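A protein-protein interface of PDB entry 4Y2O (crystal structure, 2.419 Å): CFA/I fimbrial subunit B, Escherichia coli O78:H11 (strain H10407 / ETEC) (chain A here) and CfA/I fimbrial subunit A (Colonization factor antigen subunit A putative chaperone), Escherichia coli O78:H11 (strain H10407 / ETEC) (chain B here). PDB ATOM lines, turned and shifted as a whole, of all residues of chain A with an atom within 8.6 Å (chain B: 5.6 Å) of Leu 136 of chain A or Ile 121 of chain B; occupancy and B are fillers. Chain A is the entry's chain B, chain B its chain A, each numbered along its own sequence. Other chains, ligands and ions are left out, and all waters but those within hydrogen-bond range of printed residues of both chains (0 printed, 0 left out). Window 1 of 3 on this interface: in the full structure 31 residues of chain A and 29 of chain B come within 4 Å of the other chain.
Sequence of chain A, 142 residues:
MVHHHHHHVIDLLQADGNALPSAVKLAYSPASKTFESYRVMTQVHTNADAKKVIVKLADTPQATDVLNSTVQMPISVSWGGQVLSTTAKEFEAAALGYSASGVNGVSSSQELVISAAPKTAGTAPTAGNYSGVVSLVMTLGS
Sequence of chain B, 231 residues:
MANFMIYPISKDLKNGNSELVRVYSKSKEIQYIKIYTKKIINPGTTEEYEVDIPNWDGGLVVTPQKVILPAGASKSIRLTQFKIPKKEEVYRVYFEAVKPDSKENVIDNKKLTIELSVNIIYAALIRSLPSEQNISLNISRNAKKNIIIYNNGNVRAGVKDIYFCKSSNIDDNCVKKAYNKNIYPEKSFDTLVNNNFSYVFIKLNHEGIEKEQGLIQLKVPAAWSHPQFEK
Ile 10 of chain A touches Tyr 122 of chain B (O to CE1, 3.5 Å).
CD1 of Ile 120 of chain B touches CD2 of Leu 12 of chain A, at 3.7 Å.
Val 118 of chain B touches Val 134 of chain A (CA to O, 3.6 Å).
O of Asn 119 of chain B touches CA of Ser 135 of chain A, at 3.2 Å.
Ile 121 of chain B touches Ser 135 of chain A.
Ile 120 of chain B touches Leu 136 of chain A (C to O, 3.4 Å).
O of Ile 121 of chain B touches CA of Val 137 of chain A (3.2 Å).
Tyr 122 of chain B touches Met 138 of chain A.
CG2 of Thr 139 of chain A touches O of Ala 123 of chain B, at 2.9 Å.
Of the 11 printed residues of chain B, 7 touch a printed residue of chain A.
Along chain B the printed residues that touch a printed residue of chain A span positions 94 to 123.
Among the printed residues, no Asp or Glu carboxylate lies within 4 Å of a Lys or Arg side-chain nitrogen of the other chain.
Of the printed residues of chain B, Val 134 of chain A touches Val 118 and Asn 119.
Printed residues of chain B within 4 Å of Val 137 of chain A: Ile 121 (3.2 Å).
Of the printed residues of chain A, Tyr 94 of chain B touches Lys 56.
Glu 96 of chain B touches none of the printed residues of chain A.
Ile 121 of chain B touches four residues of chain A.
Of the printed residues of chain A, Ala 123 of chain B touches Met 138 and Thr 139.
The nearest residue of chain B that does not touch Leu 136 of chain A is Tyr 122 of chain B (5.1 Å).
The nearest printed residue of chain B that does not touch Ile 10 of chain A is Ala 123 of chain B (6.4 Å).
The backbone carbonyl oxygen (O) of Val 134 of chain A is in hydrogen-bond range of the backbone NH (N) of Asn 119 of chain B, at 2.9 Å.
The backbone NH of Ala 123 of chain B sits at hydrogen-bond distance from the backbone carbonyl oxygen of Met 138 of chain A.
The side-chain hydroxyl (OH) of Tyr 122 of chain B lies within hydrogen-bond range of the backbone NH (N) of Leu 12 of chain A (3.2 Å).
The backbone carbonyl oxygen (O) of Leu 136 of chain A sits at hydrogen-bond distance from the backbone NH (N) of Ile 121 of chain B (2.5 Å).
OH of Tyr 94 of chain B lies within hydrogen-bond range of NZ of Lys 56 of chain A, 3.3 Å away.
The backbone NH of Met 138 of chain A is in hydrogen-bond range of the backbone carbonyl oxygen of Ile 121 of chain B (2.8 Å).
The backbone carbonyl oxygen (O) of Asn 119 of chain B is in hydrogen-bond range of the backbone NH (N) of Leu 136 of chain A.
The backbone carbonyl oxygen (O) of Lys 56 of chain A lies close to the backbone NH (N) of Val 137 of chain A, at 3.2 Å.
O of Tyr 122 of chain B is in hydrogen-bond range of N of Phe 95 of chain B (2.7 Å).
The backbone carbonyl oxygen of Tyr 36 of chain B is in hydrogen-bond range of the backbone NH of Tyr 94 of chain B.
OE2 of Glu 96 of chain B is in hydrogen-bond range of ND2 of Asn 119 of chain B (3.1 Å).
The backbone NH of Ile 54 of chain A sits at hydrogen-bond distance from the backbone carbonyl oxygen of Thr 139 of chain A (3.0 Å).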
ATOM      1  N   ILE A  10     -29.977 -21.539 -17.334  1.00  0.00           N
ATOM      2  CA  ILE A  10     -28.993 -21.098 -16.370  1.00  0.00           C
ATOM      3  C   ILE A  10     -28.402 -22.288 -15.657  1.00  0.00           C
ATOM      4  O   ILE A  10     -29.130 -23.080 -15.088  1.00  0.00           O
ATOM      5  CB  ILE A  10     -29.592 -20.174 -15.319  1.00  0.00           C
ATOM      6  CG1 ILE A  10     -29.901 -18.812 -15.904  1.00  0.00           C
ATOM      7  CG2 ILE A  10     -28.641 -20.003 -14.182  1.00  0.00           C
ATOM      8  CD1 ILE A  10     -30.500 -17.882 -14.919  1.00  0.00           C
ATOM      9  N   LEU A  12     -25.127 -22.814 -12.919  1.00  0.00           N
ATOM     10  CA  LEU A  12     -24.000 -22.239 -12.218  1.00  0.00           C
ATOM     11  C   LEU A  12     -23.018 -23.316 -11.823  1.00  0.00           C
ATOM     12  O   LEU A  12     -23.366 -24.252 -11.128  1.00  0.00           O
ATOM     13  CB  LEU A  12     -24.479 -21.484 -10.986  1.00  0.00           C
ATOM     14  CG  LEU A  12     -23.452 -20.797 -10.097  1.00  0.00           C
ATOM     15  CD1 LEU A  12     -22.861 -19.602 -10.764  1.00  0.00           C
ATOM     16  CD2 LEU A  12     -24.087 -20.395  -8.818  1.00  0.00           C
ATOM     17  N   LEU A  20     -20.547 -27.174  -7.333  1.00  0.00           N
ATOM     18  CA  LEU A  20     -20.451 -26.580  -6.016  1.00  0.00           C
ATOM     19  C   LEU A  20     -20.804 -27.640  -5.005  1.00  0.00           C
ATOM     20  O   LEU A  20     -21.440 -28.624  -5.345  1.00  0.00           O
ATOM     21  CB  LEU A  20     -21.374 -25.385  -5.865  1.00  0.00           C
ATOM     22  CG  LEU A  20     -21.173 -24.229  -6.830  1.00  0.00           C
ATOM     23  CD1 LEU A  20     -21.558 -22.949  -6.173  1.00  0.00           C
ATOM     24  CD2 LEU A  20     -19.771 -24.150  -7.286  1.00  0.00           C
ATOM     25  N   THR A  42     -16.442 -18.854 -10.497  1.00  0.00           N
ATOM     26  CA  THR A  42     -17.647 -19.463 -11.021  1.00  0.00           C
ATOM     27  C   THR A  42     -17.694 -19.542 -12.524  1.00  0.00           C
ATOM     28  O   THR A  42     -16.994 -18.828 -13.227  1.00  0.00           O
ATOM     29  CB  THR A  42     -18.872 -18.702 -10.590  1.00  0.00           C
ATOM     30  OG1 THR A  42     -18.686 -17.324 -10.921  1.00  0.00           O
ATOM     31  CG2 THR A  42     -19.090 -18.853  -9.113  1.00  0.00           C
ATOM     32  N   ILE A  54     -30.766 -12.353 -12.736  1.00  0.00           N
ATOM     33  CA  ILE A  54     -30.802 -11.685 -11.452  1.00  0.00           C
ATOM     34  C   ILE A  54     -30.570 -12.661 -10.328  1.00  0.00           C
ATOM     35  O   ILE A  54     -30.856 -13.838 -10.439  1.00  0.00           O
ATOM     36  CB  ILE A  54     -32.118 -10.940 -11.232  1.00  0.00           C
ATOM     37  CG1 ILE A  54     -33.096 -11.769 -10.437  1.00  0.00           C
ATOM     38  CG2 ILE A  54     -32.739 -10.585 -12.531  1.00  0.00           C
ATOM     39  CD1 ILE A  54     -34.380 -11.081 -10.254  1.00  0.00           C
ATOM     40  N   VAL A  55     -29.993 -12.153  -9.251  1.00  0.00           N
ATOM     41  CA  VAL A  55     -29.590 -12.983  -8.136  1.00  0.00           C
ATOM     42  C   VAL A  55     -29.959 -12.353  -6.826  1.00  0.00           C
ATOM     43  O   VAL A  55     -29.539 -11.259  -6.514  1.00  0.00           O
ATOM     44  CB  VAL A  55     -28.086 -13.236  -8.122  1.00  0.00           C
ATOM     45  CG1 VAL A  55     -27.787 -14.440  -7.297  1.00  0.00           C
ATOM     46  CG2 VAL A  55     -27.551 -13.425  -9.518  1.00  0.00           C
ATOM     47  N   LYS A  56     -30.829 -13.033  -6.090  1.00  0.00           N
ATOM     48  CA  LYS A  56     -31.268 -12.596  -4.773  1.00  0.00           C
ATOM     49  C   LYS A  56     -31.419 -13.860  -3.952  1.00  0.00           C
ATOM     50  O   LYS A  56     -31.606 -14.935  -4.518  1.00  0.00           O
ATOM     51  CB  LYS A  56     -32.604 -11.863  -4.866  1.00  0.00           C
ATOM     52  CG  LYS A  56     -33.695 -12.650  -5.574  1.00  0.00           C
ATOM     53  CD  LYS A  56     -35.040 -12.473  -4.889  1.00  0.00           C
ATOM     54  CE  LYS A  56     -35.931 -13.685  -5.103  1.00  0.00           C
ATOM     55  NZ  LYS A  56     -36.630 -13.637  -6.417  1.00  0.00           N
ATOM     56  N   LEU A  57     -31.333 -13.766  -2.630  1.00  0.00           N
ATOM     57  CA  LEU A  57     -31.419 -14.984  -1.871  1.00  0.00           C
ATOM     58  C   LEU A  57     -32.677 -15.019  -1.055  1.00  0.00           C
ATOM     59  O   LEU A  57     -33.353 -14.020  -0.899  1.00  0.00           O
ATOM     60  CB  LEU A  57     -30.193 -15.182  -1.003  1.00  0.00           C
ATOM     61  CG  LEU A  57     -29.840 -14.325   0.188  1.00  0.00           C
ATOM     62  CD1 LEU A  57     -28.793 -15.052   0.970  1.00  0.00           C
ATOM     63  CD2 LEU A  57     -29.303 -13.007  -0.280  1.00  0.00           C
ATOM     64  N   ALA A  58     -32.999 -16.206  -0.571  1.00  0.00           N
ATOM     65  CA  ALA A  58     -34.327 -16.494  -0.077  1.00  0.00           C
ATOM     66  C   ALA A  58     -34.579 -15.762   1.209  1.00  0.00           C
ATOM     67  O   ALA A  58     -35.634 -15.172   1.410  1.00  0.00           O
ATOM     68  CB  ALA A  58     -34.500 -17.966   0.113  1.00  0.00           C
ATOM     69  N   ASP A  59     -33.594 -15.818   2.083  1.00  0.00           N
ATOM     70  CA  ASP A  59     -33.625 -15.058   3.308  1.00  0.00           C
ATOM     71  C   ASP A  59     -32.216 -14.716   3.714  1.00  0.00           C
ATOM     72  O   ASP A  59     -31.270 -15.371   3.294  1.00  0.00           O
ATOM     73  CB  ASP A  59     -34.320 -15.837   4.407  1.00  0.00           C
ATOM     74  CG  ASP A  59     -34.057 -17.298   4.319  1.00  0.00           C
ATOM     75  OD1 ASP A  59     -33.988 -17.818   3.197  1.00  0.00           O
ATOM     76  OD2 ASP A  59     -33.920 -17.928   5.376  1.00  0.00           O
ATOM     77  N   PRO A  61     -29.168 -15.072   5.472  1.00  0.00           N
ATOM     78  CA  PRO A  61     -28.641 -16.328   5.984  1.00  0.00           C
ATOM     79  C   PRO A  61     -28.131 -16.182   7.389  1.00  0.00           C
ATOM     80  O   PRO A  61     -27.700 -15.110   7.791  1.00  0.00           O
ATOM     81  CB  PRO A  61     -27.515 -16.641   5.022  1.00  0.00           C
ATOM     82  CG  PRO A  61     -27.052 -15.330   4.580  1.00  0.00           C
ATOM     83  CD  PRO A  61     -28.259 -14.466   4.495  1.00  0.00           C
ATOM     84  N   VAL A  77     -21.907 -11.932   1.316  1.00  0.00           N
ATOM     85  CA  VAL A  77     -21.750 -12.773   0.146  1.00  0.00           C
ATOM     86  C   VAL A  77     -21.572 -11.963  -1.113  1.00  0.00           C
ATOM     87  O   VAL A  77     -22.489 -11.285  -1.553  1.00  0.00           O
ATOM     88  CB  VAL A  77     -22.963 -13.651  -0.028  1.00  0.00           C
ATOM     89  CG1 VAL A  77     -22.755 -14.585  -1.163  1.00  0.00           C
ATOM     90  CG2 VAL A  77     -23.233 -14.407   1.236  1.00  0.00           C
ATOM     91  N   SER A  78     -20.397 -12.032  -1.707  1.00  0.00           N
ATOM     92  CA  SER A  78     -20.128 -11.178  -2.843  1.00  0.00           C
ATOM     93  C   SER A  78     -20.120 -11.943  -4.155  1.00  0.00           C
ATOM     94  O   SER A  78     -19.530 -13.003  -4.271  1.00  0.00           O
ATOM     95  CB  SER A  78     -18.797 -10.447  -2.652  1.00  0.00           C
ATOM     96  OG  SER A  78     -18.661  -9.384  -3.583  1.00  0.00           O
ATOM     97  N   TRP A  79     -20.784 -11.380  -5.147  1.00  0.00           N
ATOM     98  CA  TRP A  79     -20.778 -11.938  -6.471  1.00  0.00           C
ATOM     99  C   TRP A  79     -20.605 -10.796  -7.447  1.00  0.00           C
ATOM    100  O   TRP A  79     -21.307  -9.797  -7.371  1.00  0.00           O
ATOM    101  CB  TRP A  79     -22.074 -12.696  -6.737  1.00  0.00           C
ATOM    102  CG  TRP A  79     -21.903 -14.009  -7.451  1.00  0.00           C
ATOM    103  CD1 TRP A  79     -21.948 -15.237  -6.895  1.00  0.00           C
ATOM    104  CD2 TRP A  79     -21.670 -14.208  -8.846  1.00  0.00           C
ATOM    105  NE1 TRP A  79     -21.750 -16.196  -7.846  1.00  0.00           N
ATOM    106  CE2 TRP A  79     -21.573 -15.586  -9.056  1.00  0.00           C
ATOM    107  CE3 TRP A  79     -21.524 -13.354  -9.933  1.00  0.00           C
ATOM    108  CZ2 TRP A  79     -21.343 -16.129 -10.298  1.00  0.00           C
ATOM    109  CZ3 TRP A  79     -21.294 -13.895 -11.167  1.00  0.00           C
ATOM    110  CH2 TRP A  79     -21.206 -15.266 -11.342  1.00  0.00           C
ATOM    111  N   LEU A  84     -24.502  -9.517  -1.884  1.00  0.00           N
ATOM    112  CA  LEU A  84     -25.750 -10.155  -2.273  1.00  0.00           C
ATOM    113  C   LEU A  84     -26.778  -9.981  -1.192  1.00  0.00           C
ATOM    114  O   LEU A  84     -26.618 -10.474  -0.089  1.00  0.00           O
ATOM    115  CB  LEU A  84     -25.546 -11.638  -2.589  1.00  0.00           C
ATOM    116  CG  LEU A  84     -24.789 -11.925  -3.892  1.00  0.00           C
ATOM    117  CD1 LEU A  84     -24.881 -13.383  -4.274  1.00  0.00           C
ATOM    118  CD2 LEU A  84     -25.302 -11.059  -5.012  1.00  0.00           C
ATOM    119  N   SER A  85     -27.836  -9.261  -1.534  1.00  0.00           N
ATOM    120  CA  SER A  85     -28.881  -8.921  -0.594  1.00  0.00           C
ATOM    121  C   SER A  85     -30.120  -9.726  -0.879  1.00  0.00           C
ATOM    122  O   SER A  85     -30.284 -10.236  -1.976  1.00  0.00           O
ATOM    123  CB  SER A  85     -29.208  -7.441  -0.684  1.00  0.00           C
ATOM    124  OG  SER A  85     -29.751  -7.143  -1.951  1.00  0.00           O
ATOM    125  N   LEU A 112     -17.337 -15.944  -6.518  1.00  0.00           N
ATOM    126  CA  LEU A 112     -18.251 -15.684  -5.436  1.00  0.00           C
ATOM    127  C   LEU A 112     -17.466 -15.687  -4.170  1.00  0.00           C
ATOM    128  O   LEU A 112     -16.806 -16.666  -3.853  1.00  0.00           O
ATOM    129  CB  LEU A 112     -19.339 -16.733  -5.342  1.00  0.00           C
ATOM    130  CG  LEU A 112     -19.899 -16.869  -3.925  1.00  0.00           C
ATOM    131  CD1 LEU A 112     -21.366 -16.557  -3.901  1.00  0.00           C
ATOM    132  CD2 LEU A 112     -19.655 -18.241  -3.364  1.00  0.00           C
ATOM    133  N   VAL A 133     -27.644 -22.732   6.954  1.00  0.00           N
ATOM    134  CA  VAL A 133     -27.786 -22.832   5.513  1.00  0.00           C
ATOM    135  C   VAL A 133     -27.782 -21.474   4.802  1.00  0.00           C
ATOM    136  O   VAL A 133     -28.078 -20.436   5.393  1.00  0.00           O
ATOM    137  CB  VAL A 133     -29.098 -23.520   5.108  1.00  0.00           C
ATOM    138  CG1 VAL A 133     -29.043 -24.974   5.458  1.00  0.00           C
ATOM    139  CG2 VAL A 133     -30.256 -22.855   5.764  1.00  0.00           C
ATOM    140  N   VAL A 134     -27.451 -21.504   3.519  1.00  0.00           N
ATOM    141  CA  VAL A 134     -27.576 -20.343   2.662  1.00  0.00           C
ATOM    142  C   VAL A 134     -28.279 -20.706   1.373  1.00  0.00           C
ATOM    143  O   VAL A 134     -27.731 -21.408   0.534  1.00  0.00           O
ATOM    144  CB  VAL A 134     -26.239 -19.738   2.302  1.00  0.00           C
ATOM    145  CG1 VAL A 134     -26.430 -18.667   1.264  1.00  0.00           C
ATOM    146  CG2 VAL A 134     -25.613 -19.150   3.496  1.00  0.00           C
ATOM    147  N   SER A 135     -29.498 -20.219   1.221  1.00  0.00           N
ATOM    148  CA  SER A 135     -30.215 -20.397  -0.017  1.00  0.00           C
ATOM    149  C   SER A 135     -29.779 -19.344  -0.990  1.00  0.00           C
ATOM    150  O   SER A 135     -29.531 -18.216  -0.624  1.00  0.00           O
ATOM    151  CB  SER A 135     -31.707 -20.328   0.204  1.00  0.00           C
ATOM    152  OG  SER A 135     -32.154 -21.490   0.857  1.00  0.00           O
ATOM    153  N   LEU A 136     -29.665 -19.729  -2.239  1.00  0.00           N
ATOM    154  CA  LEU A 136     -29.208 -18.828  -3.249  1.00  0.00           C
ATOM    155  C   LEU A 136     -30.154 -18.980  -4.407  1.00  0.00           C
ATOM    156  O   LEU A 136     -30.569 -20.079  -4.720  1.00  0.00           O
ATOM    157  CB  LEU A 136     -27.780 -19.153  -3.624  1.00  0.00           C
ATOM    158  CG  LEU A 136     -27.098 -18.227  -4.600  1.00  0.00           C
ATOM    159  CD1 LEU A 136     -27.088 -16.881  -4.009  1.00  0.00           C
ATOM    160  CD2 LEU A 136     -25.703 -18.696  -4.839  1.00  0.00           C
ATOM    161  N   VAL A 137     -30.517 -17.879  -5.036  1.00  0.00           N
ATOM    162  CA  VAL A 137     -31.573 -17.922  -6.018  1.00  0.00           C
ATOM    163  C   VAL A 137     -31.167 -17.290  -7.318  1.00  0.00           C
ATOM    164  O   VAL A 137     -30.739 -16.163  -7.364  1.00  0.00           O
ATOM    165  CB  VAL A 137     -32.828 -17.241  -5.496  1.00  0.00           C
ATOM    166  CG1 VAL A 137     -33.836 -17.102  -6.580  1.00  0.00           C
ATOM    167  CG2 VAL A 137     -33.408 -18.046  -4.383  1.00  0.00           C
ATOM    168  N   MET A 138     -31.300 -18.050  -8.382  1.00  0.00           N
ATOM    169  CA  MET A 138     -31.032 -17.550  -9.700  1.00  0.00           C
ATOM    170  C   MET A 138     -32.314 -17.460 -10.502  1.00  0.00           C
ATOM    171  O   MET A 138     -33.143 -18.348 -10.441  1.00  0.00           O
ATOM    172  CB  MET A 138     -30.042 -18.452 -10.393  1.00  0.00           C
ATOM    173  CG  MET A 138     -28.635 -18.282  -9.954  1.00  0.00           C
ATOM    174  SD  MET A 138     -27.639 -17.997 -11.411  1.00  0.00           S
ATOM    175  CE  MET A 138     -26.031 -17.976 -10.676  1.00  0.00           C
ATOM    176  N   THR A 139     -32.479 -16.380 -11.245  1.00  0.00           N
ATOM    177  CA  THR A 139     -33.678 -16.198 -12.028  1.00  0.00           C
ATOM    178  C   THR A 139     -33.429 -15.277 -13.158  1.00  0.00           C
ATOM    179  O   THR A 139     -32.316 -14.891 -13.410  1.00  0.00           O
ATOM    180  CB  THR A 139     -34.826 -15.612 -11.217  1.00  0.00           C
ATOM    181  OG1 THR A 139     -34.577 -15.784  -9.824  1.00  0.00           O
ATOM    182  CG2 THR A 139     -36.082 -16.302 -11.548  1.00  0.00           C
ATOM    183  N   PHE B   4     -28.818 -29.758  -8.997  1.00  0.00           N
ATOM    184  CA  PHE B   4     -29.555 -30.047 -10.197  1.00  0.00           C
ATOM    185  C   PHE B   4     -29.625 -28.850 -11.117  1.00  0.00           C
ATOM    186  O   PHE B   4     -29.123 -27.798 -10.811  1.00  0.00           O
ATOM    187  CB  PHE B   4     -30.958 -30.506  -9.837  1.00  0.00           C
ATOM    188  CG  PHE B   4     -31.773 -29.457  -9.166  1.00  0.00           C
ATOM    189  CD1 PHE B   4     -31.629 -29.200  -7.830  1.00  0.00           C
ATOM    190  CD2 PHE B   4     -32.673 -28.721  -9.870  1.00  0.00           C
ATOM    191  CE1 PHE B   4     -32.366 -28.238  -7.228  1.00  0.00           C
ATOM    192  CE2 PHE B   4     -33.402 -27.767  -9.262  1.00  0.00           C
ATOM    193  CZ  PHE B   4     -33.252 -27.529  -7.943  1.00  0.00           C
ATOM    194  N   TYR B  36     -42.728 -24.662  -6.166  1.00  0.00           N
ATOM    195  CA  TYR B  36     -43.762 -23.748  -5.741  1.00  0.00           C
ATOM    196  C   TYR B  36     -43.780 -22.483  -6.561  1.00  0.00           C
ATOM    197  O   TYR B  36     -42.763 -22.041  -7.057  1.00  0.00           O
ATOM    198  CB  TYR B  36     -43.604 -23.405  -4.261  1.00  0.00           C
ATOM    199  CG  TYR B  36     -42.240 -22.956  -3.816  1.00  0.00           C
ATOM    200  CD1 TYR B  36     -41.885 -21.634  -3.840  1.00  0.00           C
ATOM    201  CD2 TYR B  36     -41.330 -23.857  -3.329  1.00  0.00           C
ATOM    202  CE1 TYR B  36     -40.671 -21.235  -3.419  1.00  0.00           C
ATOM    203  CE2 TYR B  36     -40.110 -23.460  -2.915  1.00  0.00           C
ATOM    204  CZ  TYR B  36     -39.785 -22.151  -2.962  1.00  0.00           C
ATOM    205  OH  TYR B  36     -38.556 -21.755  -2.550  1.00  0.00           O
ATOM    206  N   TYR B  94     -40.320 -21.822  -8.571  1.00  0.00           N
ATOM    207  CA  TYR B  94     -39.095 -22.122  -7.866  1.00  0.00           C
ATOM    208  C   TYR B  94     -38.821 -23.598  -7.808  1.00  0.00           C
ATOM    209  O   TYR B  94     -39.713 -24.389  -7.609  1.00  0.00           O
ATOM    210  CB  TYR B  94     -39.161 -21.556  -6.454  1.00  0.00           C
ATOM    211  CG  TYR B  94     -39.094 -20.059  -6.387  1.00  0.00           C
ATOM    212  CD1 TYR B  94     -40.166 -19.283  -6.747  1.00  0.00           C
ATOM    213  CD2 TYR B  94     -37.962 -19.427  -5.958  1.00  0.00           C
ATOM    214  CE1 TYR B  94     -40.102 -17.941  -6.695  1.00  0.00           C
ATOM    215  CE2 TYR B  94     -37.894 -18.084  -5.899  1.00  0.00           C
ATOM    216  CZ  TYR B  94     -38.963 -17.341  -6.268  1.00  0.00           C
ATOM    217  OH  TYR B  94     -38.888 -15.981  -6.205  1.00  0.00           O
ATOM    218  N   PHE B  95     -37.567 -23.960  -7.983  1.00  0.00           N
ATOM    219  CA  PHE B  95     -37.183 -25.345  -7.884  1.00  0.00           C
ATOM    220  C   PHE B  95     -36.158 -25.489  -6.792  1.00  0.00           C
ATOM    221  O   PHE B  95     -35.105 -24.903  -6.853  1.00  0.00           O
ATOM    222  CB  PHE B  95     -36.646 -25.847  -9.213  1.00  0.00           C
ATOM    223  CG  PHE B  95     -37.698 -26.061 -10.244  1.00  0.00           C
ATOM    224  CD1 PHE B  95     -38.249 -25.009 -10.913  1.00  0.00           C
ATOM    225  CD2 PHE B  95     -38.131 -27.315 -10.547  1.00  0.00           C
ATOM    226  CE1 PHE B  95     -39.206 -25.211 -11.836  1.00  0.00           C
ATOM    227  CE2 PHE B  95     -39.082 -27.506 -11.473  1.00  0.00           C
ATOM    228  CZ  PHE B  95     -39.619 -26.459 -12.113  1.00  0.00           C
ATOM    229  N   GLU B  96     -36.478 -26.279  -5.783  1.00  0.00           N
ATOM    230  CA  GLU B  96     -35.670 -26.309  -4.581  1.00  0.00           C
ATOM    231  C   GLU B  96     -35.424 -27.685  -4.026  1.00  0.00           C
ATOM    232  O   GLU B  96     -36.339 -28.472  -3.862  1.00  0.00           O
ATOM    233  CB  GLU B  96     -36.315 -25.463  -3.499  1.00  0.00           C
ATOM    234  CG  GLU B  96     -35.595 -25.526  -2.180  1.00  0.00           C
ATOM    235  CD  GLU B  96     -36.049 -24.472  -1.217  1.00  0.00           C
ATOM    236  OE1 GLU B  96     -37.257 -24.246  -1.123  1.00  0.00           O
ATOM    237  OE2 GLU B  96     -35.190 -23.866  -0.564  1.00  0.00           O
ATOM    238  N   VAL B 118     -25.039 -25.099   1.302  1.00  0.00           N
ATOM    239  CA  VAL B 118     -25.461 -24.138   0.310  1.00  0.00           C
ATOM    240  C   VAL B 118     -26.543 -24.696  -0.591  1.00  0.00           C
ATOM    241  O   VAL B 118     -26.329 -25.663  -1.309  1.00  0.00           O
ATOM    242  CB  VAL B 118     -24.293 -23.688  -0.524  1.00  0.00           C
ATOM    243  CG1 VAL B 118     -24.774 -22.946  -1.722  1.00  0.00           C
ATOM    244  CG2 VAL B 118     -23.419 -22.814   0.303  1.00  0.00           C
ATOM    245  N   ASN B 119     -27.714 -24.075  -0.540  1.00  0.00           N
ATOM    246  CA  ASN B 119     -28.870 -24.543  -1.288  1.00  0.00           C
ATOM    247  C   ASN B 119     -29.166 -23.641  -2.455  1.00  0.00           C
ATOM    248  O   ASN B 119     -29.791 -22.610  -2.295  1.00  0.00           O
ATOM    249  CB  ASN B 119     -30.088 -24.624  -0.380  1.00  0.00           C
ATOM    250  CG  ASN B 119     -31.245 -25.351  -1.013  1.00  0.00           C
ATOM    251  OD1 ASN B 119     -31.097 -26.010  -2.033  1.00  0.00           O
ATOM    252  ND2 ASN B 119     -32.410 -25.240  -0.403  1.00  0.00           N
ATOM    253  N   ILE B 120     -28.710 -24.028  -3.632  1.00  0.00           N
ATOM    254  CA  ILE B 120     -28.954 -23.227  -4.808  1.00  0.00           C
ATOM    255  C   ILE B 120     -30.355 -23.454  -5.323  1.00  0.00           C
ATOM    256  O   ILE B 120     -30.821 -24.575  -5.418  1.00  0.00           O
ATOM    257  CB  ILE B 120     -27.944 -23.525  -5.897  1.00  0.00           C
ATOM    258  CG1 ILE B 120     -26.596 -22.960  -5.503  1.00  0.00           C
ATOM    259  CG2 ILE B 120     -28.340 -22.873  -7.174  1.00  0.00           C
ATOM    260  CD1 ILE B 120     -25.605 -22.970  -6.610  1.00  0.00           C
ATOM    261  N   ILE B 121     -31.038 -22.362  -5.627  1.00  0.00           N
ATOM    262  CA  ILE B 121     -32.403 -22.434  -6.096  1.00  0.00           C
ATOM    263  C   ILE B 121     -32.563 -21.742  -7.435  1.00  0.00           C
ATOM    264  O   ILE B 121     -32.018 -20.679  -7.663  1.00  0.00           O
ATOM    265  CB  ILE B 121     -33.360 -21.822  -5.092  1.00  0.00           C
ATOM    266  CG1 ILE B 121     -33.065 -22.341  -3.698  1.00  0.00           C
ATOM    267  CG2 ILE B 121     -34.747 -22.197  -5.412  1.00  0.00           C
ATOM    268  CD1 ILE B 121     -33.995 -21.824  -2.667  1.00  0.00           C
ATOM    269  N   TYR B 122     -33.299 -22.381  -8.327  1.00  0.00           N
ATOM    270  CA  TYR B 122     -33.602 -21.818  -9.617  1.00  0.00           C
ATOM    271  C   TYR B 122     -35.083 -21.553  -9.709  1.00  0.00           C
ATOM    272  O   TYR B 122     -35.891 -22.368  -9.305  1.00  0.00           O
ATOM    273  CB  TYR B 122     -33.180 -22.754 -10.740  1.00  0.00           C
ATOM    274  CG  TYR B 122     -31.711 -23.006 -10.868  1.00  0.00           C
ATOM    275  CD1 TYR B 122     -30.911 -22.146 -11.566  1.00  0.00           C
ATOM    276  CD2 TYR B 122     -31.136 -24.133 -10.330  1.00  0.00           C
ATOM    277  CE1 TYR B 122     -29.593 -22.373 -11.700  1.00  0.00           C
ATOM    278  CE2 TYR B 122     -29.808 -24.369 -10.464  1.00  0.00           C
ATOM    279  CZ  TYR B 122     -29.039 -23.482 -11.150  1.00  0.00           C
ATOM    280  OH  TYR B 122     -27.700 -23.698 -11.294  1.00  0.00           O
ATOM    281  N   ALA B 123     -35.434 -20.403 -10.248  1.00  0.00           N
ATOM    282  CA  ALA B 123     -36.819 -20.073 -10.440  1.00  0.00           C
ATOM    283  C   ALA B 123     -37.064 -19.707 -11.873  1.00  0.00           C
ATOM    284  O   ALA B 123     -36.269 -19.053 -12.493  1.00  0.00           O
ATOM    285  CB  ALA B 123     -37.225 -18.972  -9.541  1.00  0.00           C
